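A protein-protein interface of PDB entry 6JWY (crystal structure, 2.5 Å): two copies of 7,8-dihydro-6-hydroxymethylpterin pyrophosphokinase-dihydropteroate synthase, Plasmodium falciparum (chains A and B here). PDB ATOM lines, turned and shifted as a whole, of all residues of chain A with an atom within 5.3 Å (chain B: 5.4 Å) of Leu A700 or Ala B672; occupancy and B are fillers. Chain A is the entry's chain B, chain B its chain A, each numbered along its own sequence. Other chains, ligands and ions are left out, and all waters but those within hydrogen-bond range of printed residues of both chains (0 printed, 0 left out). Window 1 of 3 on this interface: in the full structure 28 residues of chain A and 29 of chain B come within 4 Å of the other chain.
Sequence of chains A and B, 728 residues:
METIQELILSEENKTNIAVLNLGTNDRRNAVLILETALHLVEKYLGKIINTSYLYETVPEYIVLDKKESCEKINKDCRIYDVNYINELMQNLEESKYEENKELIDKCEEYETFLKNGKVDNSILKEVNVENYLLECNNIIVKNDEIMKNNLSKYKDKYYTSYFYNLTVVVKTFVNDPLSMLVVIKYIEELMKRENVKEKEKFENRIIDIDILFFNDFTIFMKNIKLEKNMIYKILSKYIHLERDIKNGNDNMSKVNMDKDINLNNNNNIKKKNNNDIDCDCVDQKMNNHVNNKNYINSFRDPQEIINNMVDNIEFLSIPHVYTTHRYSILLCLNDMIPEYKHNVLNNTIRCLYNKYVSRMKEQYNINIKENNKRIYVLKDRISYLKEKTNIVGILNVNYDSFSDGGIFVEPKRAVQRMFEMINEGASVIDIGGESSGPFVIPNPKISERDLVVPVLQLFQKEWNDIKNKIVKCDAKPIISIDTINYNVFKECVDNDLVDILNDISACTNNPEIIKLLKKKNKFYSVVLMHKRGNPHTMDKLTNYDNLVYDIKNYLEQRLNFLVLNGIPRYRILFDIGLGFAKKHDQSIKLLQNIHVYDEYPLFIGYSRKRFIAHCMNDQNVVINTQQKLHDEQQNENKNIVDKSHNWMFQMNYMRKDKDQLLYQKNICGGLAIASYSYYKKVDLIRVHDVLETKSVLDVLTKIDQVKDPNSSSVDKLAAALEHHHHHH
Tyr B676 touches Tyr A679 (CD1 to OH, 3.4 Å).
Ser A695 touches Cys B668.
O of Cys B668 touches CG2 of Val A696, 3.4 Å away.
Ala B672 touches Val A696.
Val A699 touches Gly B669.
Val A699 touches Ala B672.
CG1 of Val A699 touches CG1 of Ile B673, 3.7 Å away.
Ala B672 touches Leu A700 (O to CD2, 3.7 Å).
Ile A703 touches Tyr B676.
O of Leu B671 is in hydrogen-bond range of OG of Ser B675, at 3.1 Å.
The side-chain hydroxyl of Ser B677 lies within hydrogen-bond range of the backbone carbonyl oxygen of Ile B673 (2.7 Å).
O of Leu A700 is in hydrogen-bond range of OH of Tyr A678.
Hydrophobic or aromatic side chains of chain B that line the printed part of chain A: Ala B672, Ile B673 and Tyr B676.
Among the printed residues, 10 pairs touch across the chains.
Among the printed residues, no Asp or Glu carboxylate lies within 4 Å of a Lys or Arg side-chain nitrogen of the other chain.
Of the printed residues of chain B, Ser A675 touches Ser B675.
Asp A698 touches none of the printed residues of chain B.
Of the printed residues of chain B, Leu A700 touches Ala B672 (3.7 Å).
Printed residues of chain B within 4 Å of Ile A703: Tyr B676 (3.4 Å).
Printed residues of chain A within 4 Å of Gly B669: Val A699 (3.5 Å).
Of chain A, only Val A696 (3.4 Å), Val A699 (3.7 Å) and Leu A700 (3.7 Å) come within 4 Å of Ala B672.
Of the printed residues of chain A, Tyr B676 touches Tyr A679 (3.4 Å) and Ile A703 (3.4 Å).
The nearest residue of chain A that does not touch Ala B672 is Ser A675 (4.7 Å).
The side-chain hydroxyl (OG) of Ser B675 is in hydrogen-bond range of the side-chain hydroxyl (OG) of Ser A675 (2.9 Å).
Ser B675 touches its own counterpart, Ser A675.
Positions printed for both chains: 674 and 675.
Of the 10 pairs that touch across the chains among the printed residues, 1 has its exchanged pair printed and touching as well.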
ATOM      1  N   ALA A 674       0.301   9.396  23.654  1.00  0.00           N
ATOM      2  CA  ALA A 674      -0.373  10.274  22.699  1.00  0.00           C
ATOM      3  C   ALA A 674      -1.213  11.331  23.435  1.00  0.00           C
ATOM      4  O   ALA A 674      -1.218  12.508  23.054  1.00  0.00           O
ATOM      5  CB  ALA A 674      -1.213   9.469  21.726  1.00  0.00           C
ATOM      6  N   SER A 675      -1.906  10.895  24.497  1.00  0.00           N
ATOM      7  CA  SER A 675      -2.725  11.798  25.290  1.00  0.00           C
ATOM      8  C   SER A 675      -1.820  12.830  25.947  1.00  0.00           C
ATOM      9  O   SER A 675      -2.043  14.044  25.819  1.00  0.00           O
ATOM     10  CB  SER A 675      -3.528  11.066  26.323  1.00  0.00           C
ATOM     11  OG  SER A 675      -4.411  10.149  25.699  1.00  0.00           O
ATOM     12  N   TYR A 678      -0.621  15.202  23.361  1.00  0.00           N
ATOM     13  CA  TYR A 678      -1.709  16.097  23.003  1.00  0.00           C
ATOM     14  C   TYR A 678      -1.767  17.278  23.973  1.00  0.00           C
ATOM     15  O   TYR A 678      -1.859  18.428  23.530  1.00  0.00           O
ATOM     16  CB  TYR A 678      -3.059  15.366  22.929  1.00  0.00           C
ATOM     17  CG  TYR A 678      -4.200  16.337  22.805  1.00  0.00           C
ATOM     18  CD1 TYR A 678      -4.544  16.876  21.574  1.00  0.00           C
ATOM     19  CD2 TYR A 678      -4.849  16.818  23.941  1.00  0.00           C
ATOM     20  CE1 TYR A 678      -5.567  17.802  21.465  1.00  0.00           C
ATOM     21  CE2 TYR A 678      -5.860  17.757  23.844  1.00  0.00           C
ATOM     22  CZ  TYR A 678      -6.206  18.253  22.601  1.00  0.00           C
ATOM     23  OH  TYR A 678      -7.197  19.188  22.509  1.00  0.00           O
ATOM     24  N   TYR A 679      -1.691  16.994  25.288  1.00  0.00           N
ATOM     25  CA  TYR A 679      -1.803  18.037  26.298  1.00  0.00           C
ATOM     26  C   TYR A 679      -0.512  18.825  26.447  1.00  0.00           C
ATOM     27  O   TYR A 679      -0.553  19.992  26.834  1.00  0.00           O
ATOM     28  CB  TYR A 679      -2.211  17.462  27.654  1.00  0.00           C
ATOM     29  CG  TYR A 679      -3.642  16.995  27.687  1.00  0.00           C
ATOM     30  CD1 TYR A 679      -4.673  17.898  27.496  1.00  0.00           C
ATOM     31  CD2 TYR A 679      -3.964  15.655  27.862  1.00  0.00           C
ATOM     32  CE1 TYR A 679      -5.994  17.492  27.500  1.00  0.00           C
ATOM     33  CE2 TYR A 679      -5.284  15.226  27.863  1.00  0.00           C
ATOM     34  CZ  TYR A 679      -6.306  16.154  27.695  1.00  0.00           C
ATOM     35  OH  TYR A 679      -7.618  15.777  27.701  1.00  0.00           O
ATOM     36  N   SER A 695      -7.979   8.273  16.640  1.00  0.00           N
ATOM     37  CA  SER A 695      -9.225   8.193  17.382  1.00  0.00           C
ATOM     38  C   SER A 695      -9.035   8.945  18.686  1.00  0.00           C
ATOM     39  O   SER A 695      -9.886   9.732  19.093  1.00  0.00           O
ATOM     40  CB  SER A 695      -9.621   6.781  17.677  1.00  0.00           C
ATOM     41  OG  SER A 695      -9.816   6.048  16.485  1.00  0.00           O
ATOM     42  N   VAL A 696      -7.889   8.696  19.324  1.00  0.00           N
ATOM     43  CA  VAL A 696      -7.683   9.220  20.656  1.00  0.00           C
ATOM     44  C   VAL A 696      -7.550  10.736  20.548  1.00  0.00           C
ATOM     45  O   VAL A 696      -8.148  11.473  21.330  1.00  0.00           O
ATOM     46  CB  VAL A 696      -6.491   8.520  21.327  1.00  0.00           C
ATOM     47  CG1 VAL A 696      -5.999   9.219  22.592  1.00  0.00           C
ATOM     48  CG2 VAL A 696      -6.832   7.062  21.599  1.00  0.00           C
ATOM     49  N   LEU A 697      -6.833  11.196  19.522  1.00  0.00           N
ATOM     50  CA  LEU A 697      -6.616  12.629  19.367  1.00  0.00           C
ATOM     51  C   LEU A 697      -7.929  13.318  19.001  1.00  0.00           C
ATOM     52  O   LEU A 697      -8.144  14.476  19.354  1.00  0.00           O
ATOM     53  CB  LEU A 697      -5.508  12.899  18.332  1.00  0.00           C
ATOM     54  CG  LEU A 697      -4.103  12.380  18.676  1.00  0.00           C
ATOM     55  CD1 LEU A 697      -3.055  12.942  17.718  1.00  0.00           C
ATOM     56  CD2 LEU A 697      -3.717  12.675  20.124  1.00  0.00           C
ATOM     57  N   ASP A 698      -8.804  12.598  18.290  1.00  0.00           N
ATOM     58  CA  ASP A 698     -10.106  13.124  17.897  1.00  0.00           C
ATOM     59  C   ASP A 698     -10.948  13.413  19.143  1.00  0.00           C
ATOM     60  O   ASP A 698     -11.394  14.542  19.354  1.00  0.00           O
ATOM     61  CB  ASP A 698     -10.794  12.205  16.878  1.00  0.00           C
ATOM     62  CG  ASP A 698     -10.331  12.418  15.443  1.00  0.00           C
ATOM     63  OD1 ASP A 698      -9.559  13.388  15.191  1.00  0.00           O
ATOM     64  OD2 ASP A 698     -10.741  11.605  14.573  1.00  0.00           O
ATOM     65  N   VAL A 699     -11.150  12.390  19.979  1.00  0.00           N
ATOM     66  CA  VAL A 699     -11.893  12.626  21.198  1.00  0.00           C
ATOM     67  C   VAL A 699     -11.260  13.757  22.007  1.00  0.00           C
ATOM     68  O   VAL A 699     -11.957  14.674  22.414  1.00  0.00           O
ATOM     69  CB  VAL A 699     -12.122  11.346  22.020  1.00  0.00           C
ATOM     70  CG1 VAL A 699     -12.942  11.646  23.269  1.00  0.00           C
ATOM     71  CG2 VAL A 699     -12.806  10.277  21.171  1.00  0.00           C
ATOM     72  N   LEU A 700      -9.945  13.726  22.227  1.00  0.00           N
ATOM     73  CA  LEU A 700      -9.348  14.742  23.087  1.00  0.00           C
ATOM     74  C   LEU A 700      -9.613  16.126  22.512  1.00  0.00           C
ATOM     75  O   LEU A 700      -9.850  17.066  23.250  1.00  0.00           O
ATOM     76  CB  LEU A 700      -7.847  14.499  23.228  1.00  0.00           C
ATOM     77  CG  LEU A 700      -7.446  13.278  24.051  1.00  0.00           C
ATOM     78  CD1 LEU A 700      -5.938  13.100  24.014  1.00  0.00           C
ATOM     79  CD2 LEU A 700      -7.929  13.372  25.487  1.00  0.00           C
ATOM     80  N   THR A 701      -9.593  16.227  21.185  1.00  0.00           N
ATOM     81  CA  THR A 701      -9.782  17.494  20.499  1.00  0.00           C
ATOM     82  C   THR A 701     -11.186  18.026  20.786  1.00  0.00           C
ATOM     83  O   THR A 701     -11.334  19.220  21.058  1.00  0.00           O
ATOM     84  CB  THR A 701      -9.450  17.362  19.001  1.00  0.00           C
ATOM     85  OG1 THR A 701      -8.073  16.987  18.911  1.00  0.00           O
ATOM     86  CG2 THR A 701      -9.697  18.632  18.213  1.00  0.00           C
ATOM     87  N   LYS A 702     -12.186  17.130  20.740  1.00  0.00           N
ATOM     88  CA  LYS A 702     -13.576  17.487  20.993  1.00  0.00           C
ATOM     89  C   LYS A 702     -13.757  17.982  22.426  1.00  0.00           C
ATOM     90  O   LYS A 702     -14.238  19.091  22.644  1.00  0.00           O
ATOM     91  CB  LYS A 702     -14.523  16.340  20.647  1.00  0.00           C
ATOM     92  CG  LYS A 702     -14.609  16.035  19.158  1.00  0.00           C
ATOM     93  CD  LYS A 702     -15.057  17.226  18.311  1.00  0.00           C
ATOM     94  CE  LYS A 702     -14.721  17.088  16.836  1.00  0.00           C
ATOM     95  NZ  LYS A 702     -15.771  16.361  16.074  1.00  0.00           N
ATOM     96  N   ILE A 703     -13.338  17.180  23.408  1.00  0.00           N
ATOM     97  CA  ILE A 703     -13.507  17.620  24.774  1.00  0.00           C
ATOM     98  C   ILE A 703     -13.004  19.057  24.936  1.00  0.00           C
ATOM     99  O   ILE A 703     -13.532  19.802  25.766  1.00  0.00           O
ATOM    100  CB  ILE A 703     -12.867  16.598  25.719  1.00  0.00           C
ATOM    101  CG1 ILE A 703     -13.636  15.272  25.651  1.00  0.00           C
ATOM    102  CG2 ILE A 703     -12.730  17.130  27.142  1.00  0.00           C
ATOM    103  CD1 ILE A 703     -12.934  14.119  26.335  1.00  0.00           C
ATOM    104  N   ASP A 704     -12.041  19.471  24.096  1.00  0.00           N
ATOM    105  CA  ASP A 704     -11.368  20.751  24.282  1.00  0.00           C
ATOM    106  C   ASP A 704     -12.023  21.862  23.470  1.00  0.00           C
ATOM    107  O   ASP A 704     -11.796  23.034  23.748  1.00  0.00           O
ATOM    108  CB  ASP A 704      -9.874  20.691  23.952  1.00  0.00           C
ATOM    109  CG  ASP A 704      -8.980  20.453  25.154  1.00  0.00           C
ATOM    110  OD1 ASP A 704      -9.518  20.397  26.287  1.00  0.00           O
ATOM    111  OD2 ASP A 704      -7.757  20.312  24.947  1.00  0.00           O
ATOM    112  N   CYS B 668     -11.204   2.933  21.287  1.00  0.00           N
ATOM    113  CA  CYS B 668     -10.070   3.833  21.228  1.00  0.00           C
ATOM    114  C   CYS B 668     -10.453   5.174  21.847  1.00  0.00           C
ATOM    115  O   CYS B 668      -9.711   5.704  22.675  1.00  0.00           O
ATOM    116  CB  CYS B 668      -9.524   3.940  19.807  1.00  0.00           C
ATOM    117  SG  CYS B 668      -8.555   2.465  19.384  1.00  0.00           S
ATOM    118  N   GLY B 669     -11.639   5.674  21.496  1.00  0.00           N
ATOM    119  CA  GLY B 669     -12.123   6.944  22.016  1.00  0.00           C
ATOM    120  C   GLY B 669     -12.326   6.914  23.535  1.00  0.00           C
ATOM    121  O   GLY B 669     -11.993   7.874  24.236  1.00  0.00           O
ATOM    122  N   GLY B 670     -12.826   5.787  24.043  1.00  0.00           N
ATOM    123  CA  GLY B 670     -12.933   5.583  25.475  1.00  0.00           C
ATOM    124  C   GLY B 670     -11.614   5.855  26.195  1.00  0.00           C
ATOM    125  O   GLY B 670     -11.589   6.483  27.266  1.00  0.00           O
ATOM    126  N   LEU B 671     -10.513   5.370  25.587  1.00  0.00           N
ATOM    127  CA  LEU B 671      -9.201   5.491  26.196  1.00  0.00           C
ATOM    128  C   LEU B 671      -8.788   6.964  26.222  1.00  0.00           C
ATOM    129  O   LEU B 671      -8.163   7.411  27.189  1.00  0.00           O
ATOM    130  CB  LEU B 671      -8.209   4.587  25.462  1.00  0.00           C
ATOM    131  CG  LEU B 671      -8.497   3.088  25.553  1.00  0.00           C
ATOM    132  CD1 LEU B 671      -7.408   2.361  24.800  1.00  0.00           C
ATOM    133  CD2 LEU B 671      -8.583   2.584  27.003  1.00  0.00           C
ATOM    134  N   ALA B 672      -9.235   7.752  25.229  1.00  0.00           N
ATOM    135  CA  ALA B 672      -9.027   9.181  25.390  1.00  0.00           C
ATOM    136  C   ALA B 672      -9.742   9.675  26.648  1.00  0.00           C
ATOM    137  O   ALA B 672      -9.205  10.475  27.409  1.00  0.00           O
ATOM    138  CB  ALA B 672      -9.397   9.979  24.158  1.00  0.00           C
ATOM    139  N   ILE B 673     -10.952   9.172  26.900  1.00  0.00           N
ATOM    140  CA  ILE B 673     -11.711   9.726  27.999  1.00  0.00           C
ATOM    141  C   ILE B 673     -11.125   9.219  29.316  1.00  0.00           C
ATOM    142  O   ILE B 673     -11.130   9.949  30.300  1.00  0.00           O
ATOM    143  CB  ILE B 673     -13.217   9.433  27.833  1.00  0.00           C
ATOM    144  CG1 ILE B 673     -13.759  10.100  26.569  1.00  0.00           C
ATOM    145  CG2 ILE B 673     -13.996   9.860  29.068  1.00  0.00           C
ATOM    146  CD1 ILE B 673     -15.207   9.802  26.310  1.00  0.00           C
ATOM    147  N   ALA B 674     -10.592   7.988  29.312  1.00  0.00           N
ATOM    148  CA  ALA B 674      -9.757   7.504  30.408  1.00  0.00           C
ATOM    149  C   ALA B 674      -8.626   8.493  30.743  1.00  0.00           C
ATOM    150  O   ALA B 674      -8.364   8.764  31.927  1.00  0.00           O
ATOM    151  CB  ALA B 674      -9.224   6.124  30.087  1.00  0.00           C
ATOM    152  N   SER B 675      -7.967   9.042  29.706  1.00  0.00           N
ATOM    153  CA  SER B 675      -6.848   9.948  29.925  1.00  0.00           C
ATOM    154  C   SER B 675      -7.365  11.243  30.535  1.00  0.00           C
ATOM    155  O   SER B 675      -6.842  11.692  31.566  1.00  0.00           O
ATOM    156  CB  SER B 675      -6.068  10.239  28.673  1.00  0.00           C
ATOM    157  OG  SER B 675      -5.643   9.034  28.044  1.00  0.00           O
ATOM    158  N   TYR B 676      -8.420  11.799  29.905  1.00  0.00           N
ATOM    159  CA  TYR B 676      -9.038  13.025  30.390  1.00  0.00           C
ATOM    160  C   TYR B 676      -9.435  12.826  31.859  1.00  0.00           C
ATOM    161  O   TYR B 676      -9.046  13.600  32.736  1.00  0.00           O
ATOM    162  CB  TYR B 676     -10.150  13.438  29.423  1.00  0.00           C
ATOM    163  CG  TYR B 676     -10.939  14.663  29.815  1.00  0.00           C
ATOM    164  CD1 TYR B 676     -10.370  15.931  29.755  1.00  0.00           C
ATOM    165  CD2 TYR B 676     -12.263  14.564  30.248  1.00  0.00           C
ATOM    166  CE1 TYR B 676     -11.087  17.064  30.112  1.00  0.00           C
ATOM    167  CE2 TYR B 676     -12.987  15.687  30.631  1.00  0.00           C
ATOM    168  CZ  TYR B 676     -12.397  16.937  30.547  1.00  0.00           C
ATOM    169  OH  TYR B 676     -13.105  18.049  30.878  1.00  0.00           O
ATOM    170  N   SER B 677     -10.123  11.714  32.118  1.00  0.00           N
ATOM    171  CA  SER B 677     -10.533  11.325  33.453  1.00  0.00           C
ATOM    172  C   SER B 677      -9.325  11.305  34.381  1.00  0.00           C
ATOM    173  O   SER B 677      -9.414  11.775  35.525  1.00  0.00           O
ATOM    174  CB  SER B 677     -11.249   9.991  33.454  1.00  0.00           C
ATOM    175  OG  SER B 677     -12.427  10.064  32.661  1.00  0.00           O
